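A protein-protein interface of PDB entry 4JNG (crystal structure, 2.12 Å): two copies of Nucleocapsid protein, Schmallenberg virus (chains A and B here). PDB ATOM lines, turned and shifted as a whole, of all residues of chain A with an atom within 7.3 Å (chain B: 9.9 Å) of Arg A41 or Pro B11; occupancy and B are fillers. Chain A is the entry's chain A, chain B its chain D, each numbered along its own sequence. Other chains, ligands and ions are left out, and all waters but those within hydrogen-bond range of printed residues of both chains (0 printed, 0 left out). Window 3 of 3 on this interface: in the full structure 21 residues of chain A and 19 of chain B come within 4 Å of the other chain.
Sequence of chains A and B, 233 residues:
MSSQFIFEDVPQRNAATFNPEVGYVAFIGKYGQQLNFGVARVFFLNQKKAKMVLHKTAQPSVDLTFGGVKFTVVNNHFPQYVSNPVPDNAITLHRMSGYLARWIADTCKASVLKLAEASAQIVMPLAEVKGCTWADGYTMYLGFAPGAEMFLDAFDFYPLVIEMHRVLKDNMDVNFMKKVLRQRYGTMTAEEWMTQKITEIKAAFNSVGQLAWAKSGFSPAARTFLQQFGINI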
ATOM      1  N   ASN A  36     -30.767   9.273  -2.325  1.00  0.00           N
ATOM      2  CA  ASN A  36     -30.428   7.878  -2.083  1.00  0.00           C
ATOM      3  C   ASN A  36     -29.023   7.850  -1.502  1.00  0.00           C
ATOM      4  O   ASN A  36     -28.353   8.874  -1.478  1.00  0.00           O
ATOM      5  CB  ASN A  36     -30.512   7.049  -3.368  1.00  0.00           C
ATOM      6  CG  ASN A  36     -29.606   7.569  -4.462  1.00  0.00           C
ATOM      7  OD1 ASN A  36     -28.385   7.442  -4.391  1.00  0.00           O
ATOM      8  ND2 ASN A  36     -30.205   8.149  -5.494  1.00  0.00           N
ATOM      9  N   PHE A  37     -28.572   6.681  -1.064  1.00  0.00           N
ATOM     10  CA  PHE A  37     -27.275   6.559  -0.408  1.00  0.00           C
ATOM     11  C   PHE A  37     -26.082   6.846  -1.318  1.00  0.00           C
ATOM     12  O   PHE A  37     -25.011   7.191  -0.829  1.00  0.00           O
ATOM     13  CB  PHE A  37     -27.116   5.174   0.232  1.00  0.00           C
ATOM     14  CG  PHE A  37     -28.090   4.887   1.348  1.00  0.00           C
ATOM     15  CD1 PHE A  37     -28.766   5.903   2.009  1.00  0.00           C
ATOM     16  CD2 PHE A  37     -28.301   3.581   1.763  1.00  0.00           C
ATOM     17  CE1 PHE A  37     -29.643   5.622   3.039  1.00  0.00           C
ATOM     18  CE2 PHE A  37     -29.179   3.299   2.794  1.00  0.00           C
ATOM     19  CZ  PHE A  37     -29.849   4.318   3.433  1.00  0.00           C
ATOM     20  N   GLY A  38     -26.252   6.690  -2.629  1.00  0.00           N
ATOM     21  CA  GLY A  38     -25.202   7.057  -3.586  1.00  0.00           C
ATOM     22  C   GLY A  38     -25.002   8.563  -3.614  1.00  0.00           C
ATOM     23  O   GLY A  38     -23.875   9.059  -3.707  1.00  0.00           O
ATOM     24  N   VAL A  39     -26.108   9.293  -3.550  1.00  0.00           N
ATOM     25  CA  VAL A  39     -26.056  10.747  -3.557  1.00  0.00           C
ATOM     26  C   VAL A  39     -25.365  11.241  -2.285  1.00  0.00           C
ATOM     27  O   VAL A  39     -24.517  12.136  -2.351  1.00  0.00           O
ATOM     28  CB  VAL A  39     -27.464  11.364  -3.692  1.00  0.00           C
ATOM     29  CG1 VAL A  39     -27.415  12.870  -3.521  1.00  0.00           C
ATOM     30  CG2 VAL A  39     -28.061  11.010  -5.047  1.00  0.00           C
ATOM     31  N   ALA A  40     -25.706  10.654  -1.139  1.00  0.00           N
ATOM     32  CA  ALA A  40     -25.062  11.039   0.122  1.00  0.00           C
ATOM     33  C   ALA A  40     -23.609  10.571   0.147  1.00  0.00           C
ATOM     34  O   ALA A  40     -22.752  11.244   0.711  1.00  0.00           O
ATOM     35  CB  ALA A  40     -25.820  10.491   1.321  1.00  0.00           C
ATOM     36  N   ARG A  41     -23.334   9.425  -0.470  1.00  0.00           N
ATOM     37  CA  ARG A  41     -21.965   8.924  -0.553  1.00  0.00           C
ATOM     38  C   ARG A  41     -21.051   9.930  -1.244  1.00  0.00           C
ATOM     39  O   ARG A  41     -19.915  10.143  -0.830  1.00  0.00           O
ATOM     40  CB  ARG A  41     -21.917   7.598  -1.321  1.00  0.00           C
ATOM     41  CG  ARG A  41     -20.509   7.212  -1.741  1.00  0.00           C
ATOM     42  CD  ARG A  41     -20.460   5.986  -2.639  1.00  0.00           C
ATOM     43  NE  ARG A  41     -19.080   5.787  -3.058  1.00  0.00           N
ATOM     44  CZ  ARG A  41     -18.135   5.219  -2.317  1.00  0.00           C
ATOM     45  NH1 ARG A  41     -18.397   4.745  -1.100  1.00  0.00           N
ATOM     46  NH2 ARG A  41     -16.910   5.115  -2.808  1.00  0.00           N
ATOM     47  N   VAL A  42     -21.545  10.494  -2.339  1.00  0.00           N
ATOM     48  CA  VAL A  42     -20.779  11.452  -3.115  1.00  0.00           C
ATOM     49  C   VAL A  42     -20.640  12.765  -2.332  1.00  0.00           C
ATOM     50  O   VAL A  42     -19.550  13.332  -2.261  1.00  0.00           O
ATOM     51  CB  VAL A  42     -21.428  11.720  -4.482  1.00  0.00           C
ATOM     52  CG1 VAL A  42     -20.691  12.829  -5.213  1.00  0.00           C
ATOM     53  CG2 VAL A  42     -21.426  10.454  -5.331  1.00  0.00           C
ATOM     54  N   PHE A  43     -21.731  13.234  -1.737  1.00  0.00           N
ATOM     55  CA  PHE A  43     -21.646  14.450  -0.934  1.00  0.00           C
ATOM     56  C   PHE A  43     -20.501  14.379   0.068  1.00  0.00           C
ATOM     57  O   PHE A  43     -19.625  15.245   0.062  1.00  0.00           O
ATOM     58  CB  PHE A  43     -22.940  14.769  -0.190  1.00  0.00           C
ATOM     59  CG  PHE A  43     -22.830  15.987   0.671  1.00  0.00           C
ATOM     60  CD1 PHE A  43     -22.971  17.249   0.121  1.00  0.00           C
ATOM     61  CD2 PHE A  43     -22.533  15.878   2.023  1.00  0.00           C
ATOM     62  CE1 PHE A  43     -22.833  18.382   0.906  1.00  0.00           C
ATOM     63  CE2 PHE A  43     -22.398  17.002   2.808  1.00  0.00           C
ATOM     64  CZ  PHE A  43     -22.553  18.262   2.252  1.00  0.00           C
ATOM     65  N   PHE A  44     -20.500  13.347   0.910  1.00  0.00           N
ATOM     66  CA  PHE A  44     -19.578  13.313   2.058  1.00  0.00           C
ATOM     67  C   PHE A  44     -18.116  13.069   1.697  1.00  0.00           C
ATOM     68  O   PHE A  44     -17.237  13.419   2.473  1.00  0.00           O
ATOM     69  CB  PHE A  44     -20.036  12.313   3.121  1.00  0.00           C
ATOM     70  CG  PHE A  44     -21.227  12.778   3.898  1.00  0.00           C
ATOM     71  CD1 PHE A  44     -21.105  13.830   4.802  1.00  0.00           C
ATOM     72  CD2 PHE A  44     -22.469  12.177   3.735  1.00  0.00           C
ATOM     73  CE1 PHE A  44     -22.197  14.273   5.517  1.00  0.00           C
ATOM     74  CE2 PHE A  44     -23.568  12.622   4.450  1.00  0.00           C
ATOM     75  CZ  PHE A  44     -23.432  13.679   5.337  1.00  0.00           C
ATOM     76  N   LEU A  45     -17.840  12.479   0.537  1.00  0.00           N
ATOM     77  CA  LEU A  45     -16.448  12.384   0.090  1.00  0.00           C
ATOM     78  C   LEU A  45     -15.958  13.651  -0.627  1.00  0.00           C
ATOM     79  O   LEU A  45     -14.754  13.899  -0.683  1.00  0.00           O
ATOM     80  CB  LEU A  45     -16.238  11.150  -0.784  1.00  0.00           C
ATOM     81  CG  LEU A  45     -16.397   9.840  -0.004  1.00  0.00           C
ATOM     82  CD1 LEU A  45     -16.667   8.684  -0.949  1.00  0.00           C
ATOM     83  CD2 LEU A  45     -15.178   9.567   0.861  1.00  0.00           C
ATOM     84  N   ASN A  46     -16.883  14.454  -1.158  1.00  0.00           N
ATOM     85  CA  ASN A  46     -16.531  15.654  -1.917  1.00  0.00           C
ATOM     86  C   ASN A  46     -16.864  16.954  -1.190  1.00  0.00           C
ATOM     87  O   ASN A  46     -16.926  18.022  -1.802  1.00  0.00           O
ATOM     88  CB  ASN A  46     -17.224  15.624  -3.274  1.00  0.00           C
ATOM     89  CG  ASN A  46     -16.669  14.547  -4.175  1.00  0.00           C
ATOM     90  OD1 ASN A  46     -17.145  13.417  -4.172  1.00  0.00           O
ATOM     91  ND2 ASN A  46     -15.657  14.894  -4.956  1.00  0.00           N
ATOM     92  N   PHE A  66     -24.422  16.654  -6.732  1.00  0.00           N
ATOM     93  CA  PHE A  66     -23.798  15.483  -6.109  1.00  0.00           C
ATOM     94  C   PHE A  66     -24.523  14.202  -6.538  1.00  0.00           C
ATOM     95  O   PHE A  66     -25.703  14.041  -6.260  1.00  0.00           O
ATOM     96  CB  PHE A  66     -23.853  15.590  -4.586  1.00  0.00           C
ATOM     97  CG  PHE A  66     -23.076  16.743  -4.034  1.00  0.00           C
ATOM     98  CD1 PHE A  66     -21.712  16.630  -3.810  1.00  0.00           C
ATOM     99  CD2 PHE A  66     -23.704  17.943  -3.739  1.00  0.00           C
ATOM    100  CE1 PHE A  66     -20.988  17.700  -3.300  1.00  0.00           C
ATOM    101  CE2 PHE A  66     -22.984  19.013  -3.238  1.00  0.00           C
ATOM    102  CZ  PHE A  66     -21.627  18.889  -3.016  1.00  0.00           C
ATOM    103  N   LEU A 100     -28.444  15.795   5.564  1.00  0.00           N
ATOM    104  CA  LEU A 100     -28.190  14.495   4.908  1.00  0.00           C
ATOM    105  C   LEU A 100     -27.816  13.408   5.909  1.00  0.00           C
ATOM    106  O   LEU A 100     -28.282  12.276   5.797  1.00  0.00           O
ATOM    107  CB  LEU A 100     -27.116  14.598   3.818  1.00  0.00           C
ATOM    108  CG  LEU A 100     -27.496  15.245   2.483  1.00  0.00           C
ATOM    109  CD1 LEU A 100     -26.246  15.460   1.642  1.00  0.00           C
ATOM    110  CD2 LEU A 100     -28.514  14.421   1.690  1.00  0.00           C
ATOM    111  N   TRP A 103     -30.970  12.523   7.544  1.00  0.00           N
ATOM    112  CA  TRP A 103     -31.777  11.720   6.630  1.00  0.00           C
ATOM    113  C   TRP A 103     -31.320  10.259   6.655  1.00  0.00           C
ATOM    114  O   TRP A 103     -32.150   9.361   6.740  1.00  0.00           O
ATOM    115  CB  TRP A 103     -31.736  12.290   5.214  1.00  0.00           C
ATOM    116  CG  TRP A 103     -32.401  11.412   4.204  1.00  0.00           C
ATOM    117  CD1 TRP A 103     -33.738  11.273   3.994  1.00  0.00           C
ATOM    118  CD2 TRP A 103     -31.757  10.536   3.281  1.00  0.00           C
ATOM    119  NE1 TRP A 103     -33.974  10.367   2.988  1.00  0.00           N
ATOM    120  CE2 TRP A 103     -32.773   9.892   2.535  1.00  0.00           C
ATOM    121  CE3 TRP A 103     -30.421  10.224   3.012  1.00  0.00           C
ATOM    122  CZ2 TRP A 103     -32.492   8.963   1.534  1.00  0.00           C
ATOM    123  CZ3 TRP A 103     -30.141   9.304   2.018  1.00  0.00           C
ATOM    124  CH2 TRP A 103     -31.175   8.676   1.294  1.00  0.00           C
ATOM    125  N   ILE A 104     -30.006  10.038   6.616  1.00  0.00           N
ATOM    126  CA  ILE A 104     -29.452   8.685   6.648  1.00  0.00           C
ATOM    127  C   ILE A 104     -29.876   7.982   7.930  1.00  0.00           C
ATOM    128  O   ILE A 104     -30.329   6.829   7.896  1.00  0.00           O
ATOM    129  CB  ILE A 104     -27.909   8.670   6.542  1.00  0.00           C
ATOM    130  CG1 ILE A 104     -27.451   9.180   5.171  1.00  0.00           C
ATOM    131  CG2 ILE A 104     -27.365   7.257   6.740  1.00  0.00           C
ATOM    132  CD1 ILE A 104     -25.996   9.602   5.137  1.00  0.00           C
ATOM    133  N   ALA A 120     -22.499  -0.125   3.718  1.00  0.00           N
ATOM    134  CA  ALA A 120     -21.659  -0.586   2.612  1.00  0.00           C
ATOM    135  C   ALA A 120     -21.345   0.499   1.581  1.00  0.00           C
ATOM    136  O   ALA A 120     -20.347   0.393   0.874  1.00  0.00           O
ATOM    137  CB  ALA A 120     -22.291  -1.799   1.937  1.00  0.00           C
ATOM    138  N   GLN A 121     -22.171   1.543   1.510  1.00  0.00           N
ATOM    139  CA  GLN A 121     -21.988   2.620   0.526  1.00  0.00           C
ATOM    140  C   GLN A 121     -21.379   3.915   1.080  1.00  0.00           C
ATOM    141  O   GLN A 121     -20.557   4.542   0.412  1.00  0.00           O
ATOM    142  CB  GLN A 121     -23.324   2.975  -0.111  1.00  0.00           C
ATOM    143  CG  GLN A 121     -23.886   1.935  -1.049  1.00  0.00           C
ATOM    144  CD  GLN A 121     -25.262   2.336  -1.513  1.00  0.00           C
ATOM    145  OE1 GLN A 121     -26.260   2.042  -0.856  1.00  0.00           O
ATOM    146  NE2 GLN A 121     -25.323   3.043  -2.632  1.00  0.00           N
ATOM    147  N   ILE A 122     -21.780   4.313   2.285  1.00  0.00           N
ATOM    148  CA  ILE A 122     -21.457   5.656   2.807  1.00  0.00           C
ATOM    149  C   ILE A 122     -20.221   5.710   3.707  1.00  0.00           C
ATOM    150  O   ILE A 122     -20.081   4.933   4.659  1.00  0.00           O
ATOM    151  CB  ILE A 122     -22.671   6.268   3.533  1.00  0.00           C
ATOM    152  CG1 ILE A 122     -23.837   6.395   2.552  1.00  0.00           C
ATOM    153  CG2 ILE A 122     -22.335   7.638   4.122  1.00  0.00           C
ATOM    154  CD1 ILE A 122     -25.169   6.639   3.217  1.00  0.00           C
ATOM    155  N   VAL A 123     -19.348   6.671   3.404  1.00  0.00           N
ATOM    156  CA  VAL A 123     -18.084   6.847   4.088  1.00  0.00           C
ATOM    157  C   VAL A 123     -18.056   8.214   4.770  1.00  0.00           C
ATOM    158  O   VAL A 123     -18.332   9.228   4.144  1.00  0.00           O
ATOM    159  CB  VAL A 123     -16.917   6.734   3.088  1.00  0.00           C
ATOM    160  CG1 VAL A 123     -15.593   6.742   3.818  1.00  0.00           C
ATOM    161  CG2 VAL A 123     -17.040   5.451   2.270  1.00  0.00           C
ATOM    162  N   PRO A 125     -15.381  10.348   6.240  1.00  0.00           N
ATOM    163  CA  PRO A 125     -13.991  10.654   6.539  1.00  0.00           C
ATOM    164  C   PRO A 125     -13.914  11.782   7.550  1.00  0.00           C
ATOM    165  O   PRO A 125     -13.945  12.948   7.183  1.00  0.00           O
ATOM    166  CB  PRO A 125     -13.417  11.086   5.184  1.00  0.00           C
ATOM    167  CG  PRO A 125     -14.521  11.003   4.200  1.00  0.00           C
ATOM    168  CD  PRO A 125     -15.796  10.952   4.970  1.00  0.00           C
ATOM    169  N   PHE B   7     -20.234  16.921  -9.065  1.00  0.00           N
ATOM    170  CA  PHE B   7     -19.479  15.890  -8.367  1.00  0.00           C
ATOM    171  C   PHE B   7     -20.099  14.510  -8.620  1.00  0.00           C
ATOM    172  O   PHE B   7     -21.314  14.332  -8.512  1.00  0.00           O
ATOM    173  CB  PHE B   7     -19.440  16.186  -6.865  1.00  0.00           C
ATOM    174  CG  PHE B   7     -18.925  17.564  -6.528  1.00  0.00           C
ATOM    175  CD1 PHE B   7     -19.779  18.658  -6.515  1.00  0.00           C
ATOM    176  CD2 PHE B   7     -17.585  17.765  -6.226  1.00  0.00           C
ATOM    177  CE1 PHE B   7     -19.308  19.926  -6.211  1.00  0.00           C
ATOM    178  CE2 PHE B   7     -17.107  19.033  -5.916  1.00  0.00           C
ATOM    179  CZ  PHE B   7     -17.969  20.114  -5.910  1.00  0.00           C
ATOM    180  N   GLU B   8     -19.247  13.552  -8.970  1.00  0.00           N
ATOM    181  CA  GLU B   8     -19.643  12.151  -9.165  1.00  0.00           C
ATOM    182  C   GLU B   8     -18.535  11.254  -8.574  1.00  0.00           C
ATOM    183  O   GLU B   8     -17.396  11.702  -8.504  1.00  0.00           O
ATOM    184  CB  GLU B   8     -19.909  11.870 -10.659  1.00  0.00           C
ATOM    185  CG  GLU B   8     -19.270  12.783 -11.692  1.00  0.00           C
ATOM    186  CD  GLU B   8     -19.904  12.603 -13.064  1.00  0.00           C
ATOM    187  OE1 GLU B   8     -20.158  11.441 -13.467  1.00  0.00           O
ATOM    188  OE2 GLU B   8     -20.163  13.622 -13.741  1.00  0.00           O
ATOM    189  N   ASP B   9     -18.801  10.020  -8.119  1.00  0.00           N
ATOM    190  CA  ASP B   9     -20.073   9.270  -8.217  1.00  0.00           C
ATOM    191  C   ASP B   9     -20.046   7.858  -7.561  1.00  0.00           C
ATOM    192  O   ASP B   9     -21.025   7.541  -6.887  1.00  0.00           O
ATOM    193  CB  ASP B   9     -20.632   9.123  -9.646  1.00  0.00           C
ATOM    194  CG  ASP B   9     -22.141   9.335  -9.707  1.00  0.00           C
ATOM    195  OD1 ASP B   9     -22.606  10.248 -10.426  1.00  0.00           O
ATOM    196  OD2 ASP B   9     -22.866   8.583  -9.021  1.00  0.00           O
ATOM    197  N   VAL B  10     -19.041   6.968  -7.707  1.00  0.00           N
ATOM    198  CA  VAL B  10     -17.704   7.035  -8.384  1.00  0.00           C
ATOM    199  C   VAL B  10     -16.586   7.126  -7.325  1.00  0.00           C
ATOM    200  O   VAL B  10     -16.398   8.186  -6.727  1.00  0.00           O
ATOM    201  CB  VAL B  10     -17.537   8.079  -9.544  1.00  0.00           C
ATOM    202  CG1 VAL B  10     -16.101   8.594  -9.662  1.00  0.00           C
ATOM    203  CG2 VAL B  10     -17.981   7.486 -10.873  1.00  0.00           C
ATOM    204  N   PRO B  11     -15.860   6.006  -7.068  1.00  0.00           N
ATOM    205  CA  PRO B  11     -16.131   4.581  -7.336  1.00  0.00           C
ATOM    206  C   PRO B  11     -15.758   3.526  -6.244  1.00  0.00           C
ATOM    207  O   PRO B  11     -16.433   2.499  -6.150  1.00  0.00           O
ATOM    208  CB  PRO B  11     -15.259   4.332  -8.562  1.00  0.00           C
ATOM    209  CG  PRO B  11     -14.047   5.182  -8.300  1.00  0.00           C
ATOM    210  CD  PRO B  11     -14.433   6.279  -7.322  1.00  0.00           C
ATOM    211  N   GLN B  12     -14.695   3.772  -5.467  1.00  0.00           N
ATOM    212  CA  GLN B  12     -14.125   2.839  -4.438  1.00  0.00           C
ATOM    213  C   GLN B  12     -13.389   1.619  -5.035  1.00  0.00           C
ATOM    214  O   GLN B  12     -14.074   0.712  -5.499  1.00  0.00           O
ATOM    215  CB  GLN B  12     -15.177   2.381  -3.413  1.00  0.00           C
ATOM    216  CG  GLN B  12     -14.632   2.148  -1.991  1.00  0.00           C
ATOM    217  CD  GLN B  12     -14.512   3.414  -1.127  1.00  0.00           C
ATOM    218  OE1 GLN B  12     -15.123   4.444  -1.413  1.00  0.00           O
ATOM    219  NE2 GLN B  12     -13.730   3.328  -0.049  1.00  0.00           N
ATOM    220  N   ARG B  13     -12.048   1.514  -5.064  1.00  0.00           N
ATOM    221  CA  ARG B  13     -10.976   2.408  -4.541  1.00  0.00           C
ATOM    222  C   ARG B  13      -9.847   1.608  -3.831  1.00  0.00           C
ATOM    223  O   ARG B  13      -8.856   2.196  -3.378  1.00  0.00           O
ATOM    224  CB  ARG B  13     -11.449   3.507  -3.592  1.00  0.00           C
ATOM    225  CG  ARG B  13     -12.031   4.771  -4.227  1.00  0.00           C
ATOM    226  CD  ARG B  13     -10.989   5.776  -4.657  1.00  0.00           C
ATOM    227  NE  ARG B  13     -10.506   5.473  -5.998  1.00  0.00           N
ATOM    228  CZ  ARG B  13      -9.565   6.162  -6.630  1.00  0.00           C
ATOM    229  NH1 ARG B  13      -8.987   7.213  -6.050  1.00  0.00           N
ATOM    230  NH2 ARG B  13      -9.200   5.797  -7.853  1.00  0.00           N
ATOM    231  N   ASN B  14     -10.002   0.287  -3.729  1.00  0.00           N
ATOM    232  CA  ASN B  14      -9.001  -0.582  -3.103  1.00  0.00           C
ATOM    233  C   ASN B  14      -8.089  -1.150  -4.182  1.00  0.00           C
ATOM    234  O   ASN B  14      -8.481  -1.217  -5.349  1.00  0.00           O
ATOM    235  CB  ASN B  14      -9.660  -1.743  -2.348  1.00  0.00           C
ATOM    236  CG  ASN B  14     -11.026  -1.384  -1.782  1.00  0.00           C
ATOM    237  OD1 ASN B  14     -11.126  -0.708  -0.762  1.00  0.00           O
ATOM    238  ND2 ASN B  14     -12.085  -1.846  -2.444  1.00  0.00           N
ATOM    239  N   SER B  83      -7.776  14.747  -6.790  1.00  0.00           N
ATOM    240  CA  SER B  83      -8.092  13.332  -7.019  1.00  0.00           C
ATOM    241  C   SER B  83      -8.662  13.215  -8.431  1.00  0.00           C
ATOM    242  O   SER B  83      -9.406  14.102  -8.852  1.00  0.00           O
ATOM    243  CB  SER B  83      -9.109  12.822  -5.999  1.00  0.00           C
ATOM    244  OG  SER B  83     -10.438  13.056  -6.439  1.00  0.00           O
ATOM    245  N   ASN B  84      -8.339  12.128  -9.144  1.00  0.00           N
ATOM    246  CA  ASN B  84      -8.629  11.998 -10.591  1.00  0.00           C
ATOM    247  C   ASN B  84      -7.792  10.864 -11.212  1.00  0.00           C
ATOM    248  O   ASN B  84      -6.572  10.860 -11.063  1.00  0.00           O
ATOM    249  CB  ASN B  84      -8.323  13.334 -11.295  1.00  0.00           C
ATOM    250  CG  ASN B  84      -8.594  13.315 -12.789  1.00  0.00           C
ATOM    251  OD1 ASN B  84      -8.359  12.324 -13.478  1.00  0.00           O
ATOM    252  ND2 ASN B  84      -9.065  14.448 -13.305  1.00  0.00           N
ATOM    253  N   PRO B  85      -8.433   9.914 -11.928  1.00  0.00           N
ATOM    254  CA  PRO B  85      -7.744   8.679 -12.345  1.00  0.00           C
ATOM    255  C   PRO B  85      -6.566   8.859 -13.313  1.00  0.00           C
ATOM    256  O   PRO B  85      -6.755   9.329 -14.438  1.00  0.00           O
ATOM    257  CB  PRO B  85      -8.858   7.871 -13.027  1.00  0.00           C
ATOM    258  CG  PRO B  85      -9.816   8.902 -13.511  1.00  0.00           C
ATOM    259  CD  PRO B  85      -9.824   9.940 -12.425  1.00  0.00           C
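The guanidinium group of Arg A41 lies close to the side-chain amide oxygen of Gln B12, 3.3 Å away.
The backbone carbonyl oxygen (O) of Gln A121 sits at hydrogen-bond distance from the guanidinium group (NH1) of Arg A41.
OD1 of Asn A46 sits close to O of Val A42 (3.1 Å).
Among the printed residues, pairs that only touch across the chains: Val A42 with Asp B9, Phe A66 with Phe B7, Asn A46 with Phe B7, Val A42 with Phe B7 and Arg A41 with Pro B11.
Of the printed residues of chain A, Pro B11 touches Arg A41.
Ala A40 touches none of the printed residues of chain B.
Val A42 touches two residues of chain B.
Of the printed residues of chain A, Phe B7 touches Val A42 (3.7 Å), Asn A46 (3.7 Å) and Phe A66 (3.6 Å).
Of the printed residues of chain B, Phe A66 touches Phe B7 (3.6 Å).
Printed residues of chain B within 4 Å of Asn A46: Phe B7.
Printed residues of chain A within 4 Å of Asp B9: Val A42.
Printed residues of chain A within 4 Å of Gln B12: Arg A41.
Among the printed residues, no Asp or Glu carboxylate lies within 4 Å of a Lys or Arg side-chain nitrogen of the other chain.
No position is printed for both chains.
Of the 6 pairs that touch across the chains among the printed residues, none has its exchanged pair printed and touching as well.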
